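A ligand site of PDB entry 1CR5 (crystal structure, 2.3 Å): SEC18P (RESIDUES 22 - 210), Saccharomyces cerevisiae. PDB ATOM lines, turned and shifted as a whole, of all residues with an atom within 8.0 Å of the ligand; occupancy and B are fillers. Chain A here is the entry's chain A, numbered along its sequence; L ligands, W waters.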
ATOM      1  N   SER A  11      12.701  12.241  16.158  1.00  0.00           N
ATOM      2  CA  SER A  11      12.653  12.343  17.617  1.00  0.00           C
ATOM      3  C   SER A  11      12.858  13.804  17.961  1.00  0.00           C
ATOM      4  O   SER A  11      13.424  14.567  17.171  1.00  0.00           O
ATOM      5  CB  SER A  11      13.760  11.512  18.260  1.00  0.00           C
ATOM      6  OG  SER A  11      15.029  12.041  17.949  1.00  0.00           O
ATOM      7  N   ASN A  12      12.387  14.201  19.139  1.00  0.00           N
ATOM      8  CA  ASN A  12      12.519  15.583  19.601  1.00  0.00           C
ATOM      9  C   ASN A  12      13.965  15.815  20.042  1.00  0.00           C
ATOM     10  O   ASN A  12      14.590  14.923  20.615  1.00  0.00           O
ATOM     11  CB  ASN A  12      11.556  15.846  20.756  1.00  0.00           C
ATOM     12  CG  ASN A  12      11.558  17.294  21.189  1.00  0.00           C
ATOM     13  OD1 ASN A  12      11.464  18.205  20.373  1.00  0.00           O
ATOM     14  ND2 ASN A  12      11.649  17.525  22.504  1.00  0.00           N
ATOM     15  N   CYS A  13      14.484  17.000  19.766  1.00  0.00           N
ATOM     16  CA  CYS A  13      15.864  17.350  20.129  1.00  0.00           C
ATOM     17  C   CYS A  13      15.807  18.773  20.661  1.00  0.00           C
ATOM     18  O   CYS A  13      16.108  19.738  19.943  1.00  0.00           O
ATOM     19  CB  CYS A  13      16.762  17.291  18.894  1.00  0.00           C
ATOM     20  SG  CYS A  13      18.545  17.489  19.160  1.00  0.00           S
ATOM     21  N   PRO A  14      15.403  18.938  21.924  1.00  0.00           N
ATOM     22  CA  PRO A  14      15.298  20.246  22.558  1.00  0.00           C
ATOM     23  C   PRO A  14      16.581  20.820  23.181  1.00  0.00           C
ATOM     24  O   PRO A  14      16.583  21.968  23.628  1.00  0.00           O
ATOM     25  CB  PRO A  14      14.223  20.007  23.603  1.00  0.00           C
ATOM     26  CG  PRO A  14      14.586  18.631  24.108  1.00  0.00           C
ATOM     27  CD  PRO A  14      14.919  17.870  22.830  1.00  0.00           C
ATOM     28  N   ASN A  15      17.659  20.039  23.237  1.00  0.00           N
ATOM     29  CA  ASN A  15      18.899  20.525  23.830  1.00  0.00           C
ATOM     30  C   ASN A  15      19.412  21.703  23.008  1.00  0.00           C
ATOM     31  O   ASN A  15      19.585  21.589  21.803  1.00  0.00           O
ATOM     32  CB  ASN A  15      19.950  19.409  23.874  1.00  0.00           C
ATOM     33  CG  ASN A  15      21.290  19.895  24.381  1.00  0.00           C
ATOM     34  OD1 ASN A  15      22.120  20.362  23.599  1.00  0.00           O
ATOM     35  ND2 ASN A  15      21.493  19.801  25.684  1.00  0.00           N
ATOM     36  N   ASN A  16      19.673  22.840  23.663  1.00  0.00           N
ATOM     37  CA  ASN A  16      20.130  24.042  22.961  1.00  0.00           C
ATOM     38  C   ASN A  16      21.363  23.943  22.063  1.00  0.00           C
ATOM     39  O   ASN A  16      21.555  24.785  21.185  1.00  0.00           O
ATOM     40  CB  ASN A  16      20.310  25.220  23.931  1.00  0.00           C
ATOM     41  CG  ASN A  16      21.076  24.841  25.179  1.00  0.00           C
ATOM     42  OD1 ASN A  16      21.817  23.863  25.201  1.00  0.00           O
ATOM     43  ND2 ASN A  16      20.893  25.627  26.238  1.00  0.00           N
ATOM     44  N   SER A  17      22.220  22.950  22.286  1.00  0.00           N
ATOM     45  CA  SER A  17      23.404  22.825  21.422  1.00  0.00           C
ATOM     46  C   SER A  17      22.948  22.471  20.005  1.00  0.00           C
ATOM     47  O   SER A  17      23.636  22.765  19.028  1.00  0.00           O
ATOM     48  CB  SER A  17      24.326  21.722  21.940  1.00  0.00           C
ATOM     49  OG  SER A  17      25.292  22.255  22.834  1.00  0.00           O
ATOM     50  N   TYR A  18      21.766  21.866  19.914  1.00  0.00           N
ATOM     51  CA  TYR A  18      21.218  21.475  18.618  1.00  0.00           C
ATOM     52  C   TYR A  18      20.040  22.355  18.207  1.00  0.00           C
ATOM     53  O   TYR A  18      20.023  22.909  17.122  1.00  0.00           O
ATOM     54  CB  TYR A  18      20.749  20.023  18.654  1.00  0.00           C
ATOM     55  CG  TYR A  18      21.820  19.036  18.984  1.00  0.00           C
ATOM     56  CD1 TYR A  18      22.246  18.830  20.296  1.00  0.00           C
ATOM     57  CD2 TYR A  18      22.428  18.283  17.976  1.00  0.00           C
ATOM     58  CE1 TYR A  18      23.247  17.906  20.604  1.00  0.00           C
ATOM     59  CE2 TYR A  18      23.425  17.364  18.277  1.00  0.00           C
ATOM     60  CZ  TYR A  18      23.824  17.185  19.582  1.00  0.00           C
ATOM     61  OH  TYR A  18      24.805  16.278  19.873  1.00  0.00           O
ATOM     62  N   ALA A  19      19.057  22.463  19.098  1.00  0.00           N
ATOM     63  CA  ALA A  19      17.839  23.230  18.843  1.00  0.00           C
ATOM     64  C   ALA A  19      18.024  24.657  18.321  1.00  0.00           C
ATOM     65  O   ALA A  19      17.162  25.154  17.596  1.00  0.00           O
ATOM     66  CB  ALA A  19      16.968  23.237  20.107  1.00  0.00           C
ATOM     67  N   VAL A  23      20.081  22.349  12.966  1.00  0.00           N
ATOM     68  CA  VAL A  23      20.737  21.225  12.335  1.00  0.00           C
ATOM     69  C   VAL A  23      19.865  20.000  12.485  1.00  0.00           C
ATOM     70  O   VAL A  23      18.850  20.038  13.184  1.00  0.00           O
ATOM     71  CB  VAL A  23      22.106  20.926  12.985  1.00  0.00           C
ATOM     72  CG1 VAL A  23      23.043  22.143  12.848  1.00  0.00           C
ATOM     73  CG2 VAL A  23      21.920  20.565  14.449  1.00  0.00           C
ATOM     74  N   ALA A  24      20.260  18.942  11.801  1.00  0.00           N
ATOM     75  CA  ALA A  24      19.550  17.668  11.892  1.00  0.00           C
ATOM     76  C   ALA A  24      20.477  16.792  12.725  1.00  0.00           C
ATOM     77  O   ALA A  24      21.580  16.461  12.287  1.00  0.00           O
ATOM     78  CB  ALA A  24      19.370  17.052  10.502  1.00  0.00           C
ATOM     79  N   ALA A  25      20.054  16.458  13.939  1.00  0.00           N
ATOM     80  CA  ALA A  25      20.868  15.624  14.814  1.00  0.00           C
ATOM     81  C   ALA A  25      20.840  14.188  14.295  1.00  0.00           C
ATOM     82  O   ALA A  25      19.765  13.588  14.189  1.00  0.00           O
ATOM     83  CB  ALA A  25      20.322  15.675  16.236  1.00  0.00           C
ATOM     84  N   VAL A  26      22.009  13.649  13.962  1.00  0.00           N
ATOM     85  CA  VAL A  26      22.069  12.272  13.452  1.00  0.00           C
ATOM     86  C   VAL A  26      23.108  11.443  14.177  1.00  0.00           C
ATOM     87  O   VAL A  26      24.001  11.975  14.847  1.00  0.00           O
ATOM     88  CB  VAL A  26      22.430  12.251  11.950  1.00  0.00           C
ATOM     89  CG1 VAL A  26      21.402  13.024  11.147  1.00  0.00           C
ATOM     90  CG2 VAL A  26      23.819  12.821  11.743  1.00  0.00           C
ATOM     91  N   ARG A  48      24.503  17.083  12.107  1.00  0.00           N
ATOM     92  CA  ARG A  48      25.333  17.221  13.282  1.00  0.00           C
ATOM     93  C   ARG A  48      25.311  15.928  14.056  1.00  0.00           C
ATOM     94  O   ARG A  48      24.252  15.445  14.467  1.00  0.00           O
ATOM     95  CB  ARG A  48      24.898  18.333  14.212  1.00  0.00           C
ATOM     96  CG  ARG A  48      25.744  18.288  15.483  1.00  0.00           C
ATOM     97  CD  ARG A  48      25.718  19.561  16.254  1.00  0.00           C
ATOM     98  NE  ARG A  48      26.137  20.688  15.432  1.00  0.00           N
ATOM     99  CZ  ARG A  48      26.167  21.933  15.883  1.00  0.00           C
ATOM    100  NH1 ARG A  48      25.812  22.162  17.129  1.00  0.00           N
ATOM    101  NH2 ARG A  48      26.540  22.939  15.089  1.00  0.00           N
ATOM    102  N   HIS A  49      26.491  15.365  14.256  1.00  0.00           N
ATOM    103  CA  HIS A  49      26.602  14.126  14.998  1.00  0.00           C
ATOM    104  C   HIS A  49      26.165  14.318  16.442  1.00  0.00           C
ATOM    105  O   HIS A  49      26.319  15.398  17.014  1.00  0.00           O
ATOM    106  CB  HIS A  49      28.056  13.631  14.971  1.00  0.00           C
ATOM    107  CG  HIS A  49      28.414  12.885  13.734  1.00  0.00           C
ATOM    108  ND1 HIS A  49      29.714  12.495  13.459  1.00  0.00           N
ATOM    109  CD2 HIS A  49      27.661  12.439  12.704  1.00  0.00           C
ATOM    110  CE1 HIS A  49      29.733  11.833  12.312  1.00  0.00           C
ATOM    111  NE2 HIS A  49      28.504  11.785  11.837  1.00  0.00           N
ATOM    112  N   SER A  50      25.613  13.253  17.012  1.00  0.00           N
ATOM    113  CA  SER A  50      25.164  13.224  18.385  1.00  0.00           C
ATOM    114  C   SER A  50      25.371  11.800  18.884  1.00  0.00           C
ATOM    115  O   SER A  50      24.989  10.838  18.214  1.00  0.00           O
ATOM    116  CB  SER A  50      23.676  13.570  18.480  1.00  0.00           C
ATOM    117  OG  SER A  50      23.159  13.185  19.735  1.00  0.00           O
ATOM    118  N   ASN A  51      25.991  11.670  20.049  1.00  0.00           N
ATOM    119  CA  ASN A  51      26.229  10.352  20.616  1.00  0.00           C
ATOM    120  C   ASN A  51      25.030   9.887  21.439  1.00  0.00           C
ATOM    121  O   ASN A  51      24.955   8.734  21.839  1.00  0.00           O
ATOM    122  CB  ASN A  51      27.479  10.358  21.505  1.00  0.00           C
ATOM    123  CG  ASN A  51      28.755  10.613  20.722  1.00  0.00           C
ATOM    124  OD1 ASN A  51      28.973  10.051  19.654  1.00  0.00           O
ATOM    125  ND2 ASN A  51      29.621  11.468  21.273  1.00  0.00           N
ATOM    126  N   ASP A  52      24.097  10.817  21.683  1.00  0.00           N
ATOM    127  CA  ASP A  52      22.901  10.496  22.466  1.00  0.00           C
ATOM    128  C   ASP A  52      21.679  10.287  21.595  1.00  0.00           C
ATOM    129  O   ASP A  52      20.546  10.414  22.070  1.00  0.00           O
ATOM    130  CB  ASP A  52      22.616  11.603  23.475  1.00  0.00           C
ATOM    131  CG  ASP A  52      23.844  12.012  24.249  1.00  0.00           C
ATOM    132  OD1 ASP A  52      24.518  11.121  24.809  1.00  0.00           O
ATOM    133  OD2 ASP A  52      24.128  13.236  24.304  1.00  0.00           O
ATOM    134  N   ILE A  53      21.887   9.984  20.319  1.00  0.00           N
ATOM    135  CA  ILE A  53      20.781   9.755  19.409  1.00  0.00           C
ATOM    136  C   ILE A  53      20.900   8.363  18.784  1.00  0.00           C
ATOM    137  O   ILE A  53      21.849   8.072  18.061  1.00  0.00           O
ATOM    138  CB  ILE A  53      20.726  10.852  18.314  1.00  0.00           C
ATOM    139  CG1 ILE A  53      19.457  10.688  17.478  1.00  0.00           C
ATOM    140  CG2 ILE A  53      21.963  10.772  17.442  1.00  0.00           C
ATOM    141  CD1 ILE A  53      19.235  11.806  16.494  1.00  0.00           C
ATOM    142  N   PRO A  54      19.918   7.490  19.066  1.00  0.00           N
ATOM    143  CA  PRO A  54      19.871   6.108  18.571  1.00  0.00           C
ATOM    144  C   PRO A  54      20.081   5.969  17.074  1.00  0.00           C
ATOM    145  O   PRO A  54      19.438   6.657  16.280  1.00  0.00           O
ATOM    146  CB  PRO A  54      18.464   5.658  18.980  1.00  0.00           C
ATOM    147  CG  PRO A  54      18.202   6.439  20.220  1.00  0.00           C
ATOM    148  CD  PRO A  54      18.717   7.802  19.851  1.00  0.00           C
ATOM    149  N   ILE A  58      16.514  10.468  13.861  1.00  0.00           N
ATOM    150  CA  ILE A  58      17.007  11.787  13.496  1.00  0.00           C
ATOM    151  C   ILE A  58      16.269  12.801  14.367  1.00  0.00           C
ATOM    152  O   ILE A  58      15.039  12.782  14.445  1.00  0.00           O
ATOM    153  CB  ILE A  58      16.779  12.073  11.984  1.00  0.00           C
ATOM    154  CG1 ILE A  58      17.374  13.420  11.612  1.00  0.00           C
ATOM    155  CG2 ILE A  58      15.284  12.029  11.648  1.00  0.00           C
ATOM    156  CD1 ILE A  58      17.351  13.695  10.114  1.00  0.00           C
ATOM    157  N   GLY A  59      17.029  13.676  15.034  1.00  0.00           N
ATOM    158  CA  GLY A  59      16.419  14.653  15.928  1.00  0.00           C
ATOM    159  C   GLY A  59      16.221  16.050  15.388  1.00  0.00           C
ATOM    160  O   GLY A  59      17.111  16.634  14.763  1.00  0.00           O
ATOM    161  N   PHE A  60      15.044  16.598  15.648  1.00  0.00           N
ATOM    162  CA  PHE A  60      14.684  17.932  15.191  1.00  0.00           C
ATOM    163  C   PHE A  60      13.962  18.668  16.320  1.00  0.00           C
ATOM    164  O   PHE A  60      13.365  18.039  17.191  1.00  0.00           O
ATOM    165  CB  PHE A  60      13.742  17.844  13.980  1.00  0.00           C
ATOM    166  CG  PHE A  60      14.399  17.373  12.707  1.00  0.00           C
ATOM    167  CD1 PHE A  60      13.964  16.237  12.054  1.00  0.00           C
ATOM    168  CD2 PHE A  60      15.424  18.111  12.128  1.00  0.00           C
ATOM    169  CE1 PHE A  60      14.517  15.833  10.838  1.00  0.00           C
ATOM    170  CE2 PHE A  60      16.000  17.723  10.911  1.00  0.00           C
ATOM    171  CZ  PHE A  60      15.545  16.580  10.263  1.00  0.00           C
ATOM    172  N   ASN A  61      14.032  19.990  16.322  1.00  0.00           N
ATOM    173  CA  ASN A  61      13.337  20.759  17.336  1.00  0.00           C
ATOM    174  C   ASN A  61      11.888  20.880  16.855  1.00  0.00           C
ATOM    175  O   ASN A  61      11.564  20.444  15.745  1.00  0.00           O
ATOM    176  CB  ASN A  61      13.970  22.154  17.525  1.00  0.00           C
ATOM    177  CG  ASN A  61      13.959  22.994  16.258  1.00  0.00           C
ATOM    178  OD1 ASN A  61      12.908  23.257  15.678  1.00  0.00           O
ATOM    179  ND2 ASN A  61      15.140  23.448  15.840  1.00  0.00           N
HETATM  180  O1  LIG L   1      18.172  17.141  22.343  1.00  0.00           O
HETATM  181  N1  LIG L   1      20.121  15.913  22.323  1.00  0.00           N
HETATM  182  C1  LIG L   1      18.958  16.110  20.305  1.00  0.00           C
HETATM  183  O2  LIG L   1      21.993  14.754  21.633  1.00  0.00           O
HETATM  184  C2  LIG L   1      18.987  16.473  21.746  1.00  0.00           C
HETATM  185  C3  LIG L   1      20.951  15.326  21.391  1.00  0.00           C
HETATM  186  C4  LIG L   1      20.350  15.548  19.996  1.00  0.00           C
HETATM  187  C5  LIG L   1      20.426  15.950  23.755  1.00  0.00           C
HETATM  188  C6  LIG L   1      19.885  14.737  24.509  1.00  0.00           C
HETATM  189  O   HOH W   1      16.763  13.527  19.639  1.00  0.00           O
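Water W1 bridges the backbone carbonyl oxygen (O) of Asn 12 and the side-chain hydroxyl (OG) of Ser 11.
The backbone NH (N) of Gly 59 sits at hydrogen-bond distance from the backbone carbonyl oxygen (O) of Ala 25 (2.9 Å).
The side-chain amide oxygen of Asn 15 is in hydrogen-bond range of the backbone NH of Ser 17.
The backbone carbonyl oxygen (O) of Phe 60 lies within hydrogen-bond range of the backbone NH (N) of Cys 13.
The backbone NH of Ser 50 is in hydrogen-bond range of the backbone carbonyl oxygen of Val 26.
The backbone NH (N) of Asp 52 is in hydrogen-bond range of the side-chain hydroxyl (OG) of Ser 50, 3.2 Å away.
The side-chain hydroxyl (OG) of Ser 50 sits at hydrogen-bond distance from the backbone NH (N) of Ile 53.
The backbone carbonyl oxygen of His 49 sits at hydrogen-bond distance from the side-chain hydroxyl of Tyr 18 (3.4 Å).
The side-chain hydroxyl of Ser 50 is in hydrogen-bond range of an oxygen (O2) of the ligand.
The backbone NH (N) of Asn 15 is in hydrogen-bond range of an oxygen (O1) of the ligand (3.1 Å).
C1 of the ligand is bonded to SG of Cys 13 (1.8 Å).
The backbone nitrogen (N) of Pro 14 lies close to an oxygen (O1) of the ligand, at 3.3 Å.
Tyr 18 touches the ligand.
Ala 25 touches the ligand (CB to C4, 3.8 Å).
Asp 52 touches the ligand (CB to O2, 3.7 Å).
Hydrophobic or aromatic side chains that line the ligand: Pro 14, Tyr 18 and Ala 25.
Of the 24 residues printed, 7 come within 4 Å of the ligand.
The nearest printed residue that does not touch the ligand is Asn 12 (4.5 Å).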
